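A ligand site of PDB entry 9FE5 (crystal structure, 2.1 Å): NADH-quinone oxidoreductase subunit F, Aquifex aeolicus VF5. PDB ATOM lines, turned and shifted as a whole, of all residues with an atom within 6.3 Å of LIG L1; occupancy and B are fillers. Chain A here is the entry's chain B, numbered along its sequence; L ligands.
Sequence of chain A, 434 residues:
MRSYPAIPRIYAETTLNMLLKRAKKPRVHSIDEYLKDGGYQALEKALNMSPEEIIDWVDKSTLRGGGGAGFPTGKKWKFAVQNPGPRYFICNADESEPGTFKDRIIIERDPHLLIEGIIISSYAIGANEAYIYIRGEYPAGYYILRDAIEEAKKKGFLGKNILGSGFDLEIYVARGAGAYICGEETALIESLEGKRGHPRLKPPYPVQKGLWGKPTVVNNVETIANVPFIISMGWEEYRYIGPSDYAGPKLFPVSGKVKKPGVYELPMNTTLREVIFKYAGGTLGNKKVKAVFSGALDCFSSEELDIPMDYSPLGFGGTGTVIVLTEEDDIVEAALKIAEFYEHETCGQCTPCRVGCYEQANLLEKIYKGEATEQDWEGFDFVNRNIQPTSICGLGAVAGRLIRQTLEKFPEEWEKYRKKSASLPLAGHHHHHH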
ATOM      1  N   ILE A 181      24.487  -7.228  -1.816  1.00  0.00           N
ATOM      2  CA  ILE A 181      24.157  -8.633  -1.672  1.00  0.00           C
ATOM      3  C   ILE A 181      23.821  -8.955  -0.209  1.00  0.00           C
ATOM      4  O   ILE A 181      23.120  -9.921   0.059  1.00  0.00           O
ATOM      5  CB  ILE A 181      25.286  -9.524  -2.222  1.00  0.00           C
ATOM      6  CG1 ILE A 181      24.824 -10.959  -2.416  1.00  0.00           C
ATOM      7  CG2 ILE A 181      26.524  -9.460  -1.325  1.00  0.00           C
ATOM      8  CD1 ILE A 181      23.606 -11.104  -3.315  1.00  0.00           C
ATOM      9  N   GLY A 197      29.786 -11.255   2.729  1.00  0.00           N
ATOM     10  CA  GLY A 197      28.373 -11.440   2.437  1.00  0.00           C
ATOM     11  C   GLY A 197      28.170 -12.428   1.295  1.00  0.00           C
ATOM     12  O   GLY A 197      27.876 -12.018   0.174  1.00  0.00           O
ATOM     13  N   HIS A 198      28.319 -13.721   1.592  1.00  0.00           N
ATOM     14  CA  HIS A 198      28.172 -14.769   0.601  1.00  0.00           C
ATOM     15  C   HIS A 198      26.884 -15.539   0.843  1.00  0.00           C
ATOM     16  O   HIS A 198      26.758 -16.220   1.845  1.00  0.00           O
ATOM     17  CB  HIS A 198      29.384 -15.713   0.611  1.00  0.00           C
ATOM     18  CG  HIS A 198      30.606 -15.167  -0.041  1.00  0.00           C
ATOM     19  ND1 HIS A 198      31.850 -15.737   0.117  1.00  0.00           N
ATOM     20  CD2 HIS A 198      30.775 -14.157  -0.906  1.00  0.00           C
ATOM     21  CE1 HIS A 198      32.735 -15.079  -0.606  1.00  0.00           C
ATOM     22  NE2 HIS A 198      32.107 -14.118  -1.240  1.00  0.00           N
ATOM     23  N   PRO A 199      25.882 -15.456  -0.059  1.00  0.00           N
ATOM     24  CA  PRO A 199      24.642 -16.218   0.119  1.00  0.00           C
ATOM     25  C   PRO A 199      24.890 -17.719   0.266  1.00  0.00           C
ATOM     26  O   PRO A 199      25.843 -18.271  -0.290  1.00  0.00           O
ATOM     27  CB  PRO A 199      23.836 -15.880  -1.145  1.00  0.00           C
ATOM     28  CG  PRO A 199      24.364 -14.519  -1.554  1.00  0.00           C
ATOM     29  CD  PRO A 199      25.854 -14.590  -1.254  1.00  0.00           C
ATOM     30  N   ARG A 200      23.998 -18.356   1.033  1.00  0.00           N
ATOM     31  CA  ARG A 200      23.991 -19.801   1.192  1.00  0.00           C
ATOM     32  C   ARG A 200      22.882 -20.395   0.337  1.00  0.00           C
ATOM     33  O   ARG A 200      21.820 -19.793   0.155  1.00  0.00           O
ATOM     34  CB  ARG A 200      23.700 -20.228   2.632  1.00  0.00           C
ATOM     35  CG  ARG A 200      24.501 -19.553   3.732  1.00  0.00           C
ATOM     36  CD  ARG A 200      23.878 -19.900   5.085  1.00  0.00           C
ATOM     37  NE  ARG A 200      24.618 -19.342   6.216  1.00  0.00           N
ATOM     38  CZ  ARG A 200      24.230 -19.314   7.488  1.00  0.00           C
ATOM     39  NH1 ARG A 200      23.038 -19.789   7.833  1.00  0.00           N
ATOM     40  NH2 ARG A 200      25.034 -18.811   8.414  1.00  0.00           N
ATOM     41  N   GLU A 345      27.764  -5.546  -7.984  1.00  0.00           N
ATOM     42  CA  GLU A 345      27.162  -6.175  -6.815  1.00  0.00           C
ATOM     43  C   GLU A 345      27.223  -7.709  -6.784  1.00  0.00           C
ATOM     44  O   GLU A 345      27.029  -8.283  -5.715  1.00  0.00           O
ATOM     45  CB  GLU A 345      25.726  -5.687  -6.604  1.00  0.00           C
ATOM     46  CG  GLU A 345      25.629  -4.181  -6.384  1.00  0.00           C
ATOM     47  CD  GLU A 345      26.480  -3.600  -5.275  1.00  0.00           C
ATOM     48  OE1 GLU A 345      26.906  -4.344  -4.356  1.00  0.00           O
ATOM     49  OE2 GLU A 345      26.739  -2.375  -5.347  1.00  0.00           O
ATOM     50  N   THR A 346      27.460  -8.393  -7.912  1.00  0.00           N
ATOM     51  CA  THR A 346      27.625  -9.837  -7.850  1.00  0.00           C
ATOM     52  C   THR A 346      28.719 -10.152  -6.835  1.00  0.00           C
ATOM     53  O   THR A 346      29.728  -9.454  -6.765  1.00  0.00           O
ATOM     54  CB  THR A 346      27.943 -10.432  -9.224  1.00  0.00           C
ATOM     55  OG1 THR A 346      28.125 -11.841  -9.047  1.00  0.00           O
ATOM     56  CG2 THR A 346      29.191  -9.847  -9.848  1.00  0.00           C
ATOM     57  N   CYS A 347      28.495 -11.178  -6.000  1.00  0.00           N
ATOM     58  CA  CYS A 347      29.448 -11.525  -4.967  1.00  0.00           C
ATOM     59  C   CYS A 347      30.536 -12.462  -5.496  1.00  0.00           C
ATOM     60  O   CYS A 347      31.555 -12.646  -4.828  1.00  0.00           O
ATOM     61  CB  CYS A 347      28.745 -12.143  -3.763  1.00  0.00           C
ATOM     62  SG  CYS A 347      28.362 -13.897  -3.974  1.00  0.00           S
ATOM     63  N   GLY A 348      30.278 -13.097  -6.648  1.00  0.00           N
ATOM     64  CA  GLY A 348      31.311 -13.811  -7.391  1.00  0.00           C
ATOM     65  C   GLY A 348      31.360 -15.325  -7.127  1.00  0.00           C
ATOM     66  O   GLY A 348      32.191 -16.007  -7.730  1.00  0.00           O
ATOM     67  N   GLN A 349      30.483 -15.845  -6.258  1.00  0.00           N
ATOM     68  CA  GLN A 349      30.495 -17.243  -5.860  1.00  0.00           C
ATOM     69  C   GLN A 349      30.216 -18.177  -7.038  1.00  0.00           C
ATOM     70  O   GLN A 349      30.811 -19.246  -7.147  1.00  0.00           O
ATOM     71  CB  GLN A 349      29.389 -17.563  -4.855  1.00  0.00           C
ATOM     72  CG  GLN A 349      29.777 -17.382  -3.399  1.00  0.00           C
ATOM     73  CD  GLN A 349      28.718 -17.896  -2.451  1.00  0.00           C
ATOM     74  OE1 GLN A 349      27.687 -17.243  -2.214  1.00  0.00           O
ATOM     75  NE2 GLN A 349      28.939 -19.079  -1.899  1.00  0.00           N
ATOM     76  N   CYS A 350      29.235 -17.786  -7.868  1.00  0.00           N
ATOM     77  CA  CYS A 350      28.732 -18.587  -8.964  1.00  0.00           C
ATOM     78  C   CYS A 350      29.351 -18.068 -10.260  1.00  0.00           C
ATOM     79  O   CYS A 350      29.365 -16.873 -10.502  1.00  0.00           O
ATOM     80  CB  CYS A 350      27.204 -18.531  -9.028  1.00  0.00           C
ATOM     81  SG  CYS A 350      26.384 -18.604  -7.408  1.00  0.00           S
ATOM     82  N   THR A 351      29.831 -18.982 -11.113  1.00  0.00           N
ATOM     83  CA  THR A 351      30.647 -18.588 -12.264  1.00  0.00           C
ATOM     84  C   THR A 351      29.796 -17.804 -13.263  1.00  0.00           C
ATOM     85  O   THR A 351      30.189 -16.701 -13.652  1.00  0.00           O
ATOM     86  CB  THR A 351      31.335 -19.810 -12.875  1.00  0.00           C
ATOM     87  OG1 THR A 351      32.375 -20.091 -11.942  1.00  0.00           O
ATOM     88  CG2 THR A 351      31.933 -19.559 -14.250  1.00  0.00           C
ATOM     89  N   CYS A 353      27.083 -16.018 -12.930  1.00  0.00           N
ATOM     90  CA  CYS A 353      26.749 -14.731 -12.340  1.00  0.00           C
ATOM     91  C   CYS A 353      27.987 -13.827 -12.330  1.00  0.00           C
ATOM     92  O   CYS A 353      27.927 -12.685 -12.795  1.00  0.00           O
ATOM     93  CB  CYS A 353      26.199 -14.903 -10.935  1.00  0.00           C
ATOM     94  SG  CYS A 353      25.694 -13.364 -10.100  1.00  0.00           S
ATOM     95  N   ARG A 354      29.095 -14.369 -11.813  1.00  0.00           N
ATOM     96  CA  ARG A 354      30.345 -13.631 -11.705  1.00  0.00           C
ATOM     97  C   ARG A 354      30.770 -13.060 -13.063  1.00  0.00           C
ATOM     98  O   ARG A 354      31.001 -11.856 -13.185  1.00  0.00           O
ATOM     99  CB  ARG A 354      31.460 -14.494 -11.121  1.00  0.00           C
ATOM    100  CG  ARG A 354      32.815 -13.802 -11.026  1.00  0.00           C
ATOM    101  CD  ARG A 354      33.909 -14.683 -10.428  1.00  0.00           C
ATOM    102  NE  ARG A 354      34.245 -15.838 -11.272  1.00  0.00           N
ATOM    103  CZ  ARG A 354      33.927 -17.098 -11.003  1.00  0.00           C
ATOM    104  NH1 ARG A 354      33.177 -17.379  -9.952  1.00  0.00           N
ATOM    105  NH2 ARG A 354      34.349 -18.071 -11.806  1.00  0.00           N
ATOM    106  N   CYS A 357      27.555 -10.943 -15.046  1.00  0.00           N
ATOM    107  CA  CYS A 357      27.272  -9.567 -14.662  1.00  0.00           C
ATOM    108  C   CYS A 357      28.363  -8.648 -15.208  1.00  0.00           C
ATOM    109  O   CYS A 357      28.065  -7.549 -15.688  1.00  0.00           O
ATOM    110  CB  CYS A 357      27.105  -9.415 -13.143  1.00  0.00           C
ATOM    111  SG  CYS A 357      25.656 -10.259 -12.465  1.00  0.00           S
ATOM    112  N   ILE A 387      23.255 -15.531 -17.269  1.00  0.00           N
ATOM    113  CA  ILE A 387      23.760 -15.149 -15.965  1.00  0.00           C
ATOM    114  C   ILE A 387      23.231 -16.133 -14.917  1.00  0.00           C
ATOM    115  O   ILE A 387      23.925 -16.462 -13.950  1.00  0.00           O
ATOM    116  CB  ILE A 387      23.363 -13.689 -15.639  1.00  0.00           C
ATOM    117  CG1 ILE A 387      23.742 -12.745 -16.788  1.00  0.00           C
ATOM    118  CG2 ILE A 387      23.973 -13.235 -14.304  1.00  0.00           C
ATOM    119  CD1 ILE A 387      23.458 -11.278 -16.522  1.00  0.00           C
ATOM    120  N   THR A 390      23.094 -22.123 -12.474  1.00  0.00           N
ATOM    121  CA  THR A 390      23.837 -22.572 -11.301  1.00  0.00           C
ATOM    122  C   THR A 390      23.797 -21.550 -10.165  1.00  0.00           C
ATOM    123  O   THR A 390      24.389 -21.806  -9.116  1.00  0.00           O
ATOM    124  CB  THR A 390      25.297 -22.963 -11.606  1.00  0.00           C
ATOM    125  OG1 THR A 390      26.091 -21.781 -11.576  1.00  0.00           O
ATOM    126  CG2 THR A 390      25.451 -23.714 -12.915  1.00  0.00           C
ATOM    127  N   SER A 391      23.098 -20.415 -10.349  1.00  0.00           N
ATOM    128  CA  SER A 391      23.075 -19.353  -9.350  1.00  0.00           C
ATOM    129  C   SER A 391      22.389 -19.835  -8.081  1.00  0.00           C
ATOM    130  O   SER A 391      21.388 -20.528  -8.147  1.00  0.00           O
ATOM    131  CB  SER A 391      22.394 -18.113  -9.873  1.00  0.00           C
ATOM    132  OG  SER A 391      21.063 -18.392 -10.288  1.00  0.00           O
ATOM    133  N   ILE A 392      22.917 -19.436  -6.919  1.00  0.00           N
ATOM    134  CA  ILE A 392      22.361 -19.886  -5.641  1.00  0.00           C
ATOM    135  C   ILE A 392      21.553 -18.781  -4.953  1.00  0.00           C
ATOM    136  O   ILE A 392      21.074 -19.010  -3.858  1.00  0.00           O
ATOM    137  CB  ILE A 392      23.456 -20.446  -4.703  1.00  0.00           C
ATOM    138  CG1 ILE A 392      24.496 -19.405  -4.280  1.00  0.00           C
ATOM    139  CG2 ILE A 392      24.119 -21.672  -5.340  1.00  0.00           C
ATOM    140  CD1 ILE A 392      25.763 -20.011  -3.694  1.00  0.00           C
ATOM    141  N   CYS A 393      21.393 -17.602  -5.580  1.00  0.00           N
ATOM    142  CA  CYS A 393      20.526 -16.560  -5.010  1.00  0.00           C
ATOM    143  C   CYS A 393      19.864 -15.780  -6.138  1.00  0.00           C
ATOM    144  O   CYS A 393      20.179 -15.990  -7.300  1.00  0.00           O
ATOM    145  CB  CYS A 393      21.275 -15.642  -4.045  1.00  0.00           C
ATOM    146  SG  CYS A 393      22.018 -14.176  -4.821  1.00  0.00           S
ATOM    147  N   GLY A 394      18.948 -14.868  -5.753  1.00  0.00           N
ATOM    148  CA  GLY A 394      18.068 -14.184  -6.699  1.00  0.00           C
ATOM    149  C   GLY A 394      18.797 -13.176  -7.587  1.00  0.00           C
ATOM    150  O   GLY A 394      18.302 -12.857  -8.664  1.00  0.00           O
ATOM    151  N   LEU A 395      19.948 -12.640  -7.153  1.00  0.00           N
ATOM    152  CA  LEU A 395      20.688 -11.676  -7.963  1.00  0.00           C
ATOM    153  C   LEU A 395      21.046 -12.307  -9.306  1.00  0.00           C
ATOM    154  O   LEU A 395      20.728 -11.743 -10.355  1.00  0.00           O
ATOM    155  CB  LEU A 395      21.929 -11.172  -7.232  1.00  0.00           C
ATOM    156  CG  LEU A 395      22.661  -9.978  -7.862  1.00  0.00           C
ATOM    157  CD1 LEU A 395      23.486  -9.261  -6.797  1.00  0.00           C
ATOM    158  CD2 LEU A 395      23.567 -10.371  -9.027  1.00  0.00           C
ATOM    159  N   GLY A 396      21.687 -13.480  -9.286  1.00  0.00           N
ATOM    160  CA  GLY A 396      22.024 -14.190 -10.510  1.00  0.00           C
ATOM    161  C   GLY A 396      20.777 -14.470 -11.358  1.00  0.00           C
ATOM    162  O   GLY A 396      20.795 -14.326 -12.575  1.00  0.00           O
ATOM    163  N   ALA A 397      19.683 -14.834 -10.670  1.00  0.00           N
ATOM    164  CA  ALA A 397      18.445 -15.179 -11.340  1.00  0.00           C
ATOM    165  C   ALA A 397      17.857 -13.987 -12.118  1.00  0.00           C
ATOM    166  O   ALA A 397      17.188 -14.200 -13.116  1.00  0.00           O
ATOM    167  CB  ALA A 397      17.450 -15.709 -10.336  1.00  0.00           C
HETATM  168 FE1  LIG L   1      26.706 -14.349  -5.490  1.00  0.00          FE
HETATM  169 FE2  LIG L   1      25.558 -14.087  -7.981  1.00  0.00          FE
HETATM  170 FE3  LIG L   1      23.999 -14.710  -5.789  1.00  0.00          FE
HETATM  171 FE4  LIG L   1      25.745 -16.532  -6.816  1.00  0.00          FE
HETATM  172  S1  LIG L   1      23.896 -15.679  -7.860  1.00  0.00           S
HETATM  173  S2  LIG L   1      25.419 -16.048  -4.609  1.00  0.00           S
HETATM  174  S3  LIG L   1      27.488 -15.186  -7.471  1.00  0.00           S
HETATM  175  S4  LIG L   1      25.207 -12.756  -6.129  1.00  0.00           S
HETATM  176  C1  LG2 L   2      17.038  -9.219  -1.126  1.00  0.00           C
HETATM  177  N1  LG2 L   2      16.020  -9.013  -0.144  1.00  0.00           N
HETATM  178  C2  LG2 L   2      16.001  -7.818   0.564  1.00  0.00           C
HETATM  179  N2  LG2 L   2      15.029  -7.646   1.526  1.00  0.00           N
HETATM  180  C3  LG2 L   2      15.005  -6.554   2.357  1.00  0.00           C
HETATM  181  O1  LG2 L   2      14.238  -6.484   3.316  1.00  0.00           O
HETATM  182  N3  LG2 L   2      15.913  -5.569   2.090  1.00  0.00           N
HETATM  183  C4  LG2 L   2      16.931  -5.615   1.144  1.00  0.00           C
HETATM  184  O2  LG2 L   2      17.704  -4.663   1.034  1.00  0.00           O
HETATM  185  C5  LG2 L   2      16.941  -6.830   0.371  1.00  0.00           C
HETATM  186  N4  LG2 L   2      17.941  -7.039  -0.535  1.00  0.00           N
HETATM  187  C6  LG2 L   2      18.003  -8.210  -1.293  1.00  0.00           C
HETATM  188  C7  LG2 L   2      19.038  -8.384  -2.214  1.00  0.00           C
HETATM  189  C8  LG2 L   2      19.112  -9.543  -2.990  1.00  0.00           C
HETATM  190  C9  LG2 L   2      20.229  -9.692  -3.992  1.00  0.00           C
HETATM  191  C10 LG2 L   2      18.132 -10.546  -2.829  1.00  0.00           C
HETATM  192  C11 LG2 L   2      18.159 -11.793  -3.680  1.00  0.00           C
HETATM  193  C12 LG2 L   2      17.112 -10.378  -1.902  1.00  0.00           C
HETATM  194  C13 LG2 L   2      15.043 -10.062   0.146  1.00  0.00           C
HETATM  195  C14 LG2 L   2      15.499 -10.888   1.342  1.00  0.00           C
HETATM  196  O3  LG2 L   2      16.383 -11.912   0.886  1.00  0.00           O
HETATM  197  C15 LG2 L   2      14.287 -11.489   2.064  1.00  0.00           C
HETATM  198  O4  LG2 L   2      13.386 -12.065   1.118  1.00  0.00           O
HETATM  199  C16 LG2 L   2      13.518 -10.497   2.940  1.00  0.00           C
HETATM  200  O5  LG2 L   2      14.395  -9.701   3.753  1.00  0.00           O
HETATM  201  C17 LG2 L   2      12.503 -11.205   3.807  1.00  0.00           C
HETATM  202  O6  LG2 L   2      11.687 -10.233   4.495  1.00  0.00           O
HETATM  203  P1  LG2 L   2      10.137 -10.074   4.067  1.00  0.00           P
HETATM  204  O7  LG2 L   2       9.534 -11.454   3.986  1.00  0.00           O
HETATM  205  O8  LG2 L   2      10.074  -9.347   2.731  1.00  0.00           O
HETATM  206  O9  LG2 L   2       9.590  -9.241   5.211  1.00  0.00           O
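The side-chain sulfur (SG) of Cys 350 lies close to the backbone NH (N) of Ile 392 (3.6 Å).
The backbone NH (N) of Gly 348 lies close to the side-chain hydroxyl (OG1) of Thr 346 (3.5 Å).
The backbone NH (N) of Gln 349 sits close to the side-chain sulfur (SG) of Cys 347 (3.7 Å).
SG of Cys 393 sits close to N of Leu 395 (3.5 Å).
The backbone carbonyl oxygen (O) of Gly 348 sits at hydrogen-bond distance from the guanidinium group (NH1) of Arg 354, 2.8 Å away.
OG1 of Thr 346 lies close to SG of Cys 353 (3.1 Å).
The side-chain amide oxygen of Gln 349 sits close to the backbone carbonyl oxygen of Pro 199 (2.9 Å).
N of Cys 353 is in hydrogen-bond range of O of Ile 387.
An iron atom (FE1) of LIG L1 is bound by the side-chain sulfur (SG) of Cys 347.
A sulfur (S3) of LIG L1 lies close to the backbone NH (N) of Cys 350, at 3.2 Å.
The side-chain sulfur of Cys 353 binds an iron atom (FE2) of LIG L1, 2.2 Å away.
The backbone NH (N) of Cys 347 lies close to a sulfur (S4) of LIG L1 (3.6 Å).
The side-chain hydroxyl (OG1) of Thr 346 sits close to a sulfur (S3) of LIG L1, at 3.8 Å.
SG of Cys 350 is bound to FE4 of LIG L1 (2.2 Å).
The backbone NH (N) of Gln 349 sits close to a sulfur (S3) of LIG L1, at 3.3 Å.
The backbone NH of Gly 396 sits close to a sulfur (S1) of LIG L1 (3.4 Å).
The backbone NH of Gly 348 lies close to a sulfur (S3) of LIG L1 (3.6 Å).
OE1 of Gln 349 lies close to S2 of LIG L1.
An iron atom (FE3) of LIG L1 is bound by the side-chain sulfur (SG) of Cys 393 (2.3 Å).
CD1 of Ile 181 touches S4 of LIG L1, at 3.6 Å.
Pro 199 touches LIG L1.
Ser 391 touches LIG L1.
Ile 392 touches LIG L1 (CG1 to S2, 3.5 Å).
Leu 395 touches LIG L1.
Hydrophobic or aromatic side chains within 4 Å of LIG L1: Ile 181, Pro 199, Ile 392 and Leu 395.
Of the 24 residues printed, 13 come within 4 Å of LIG L1.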
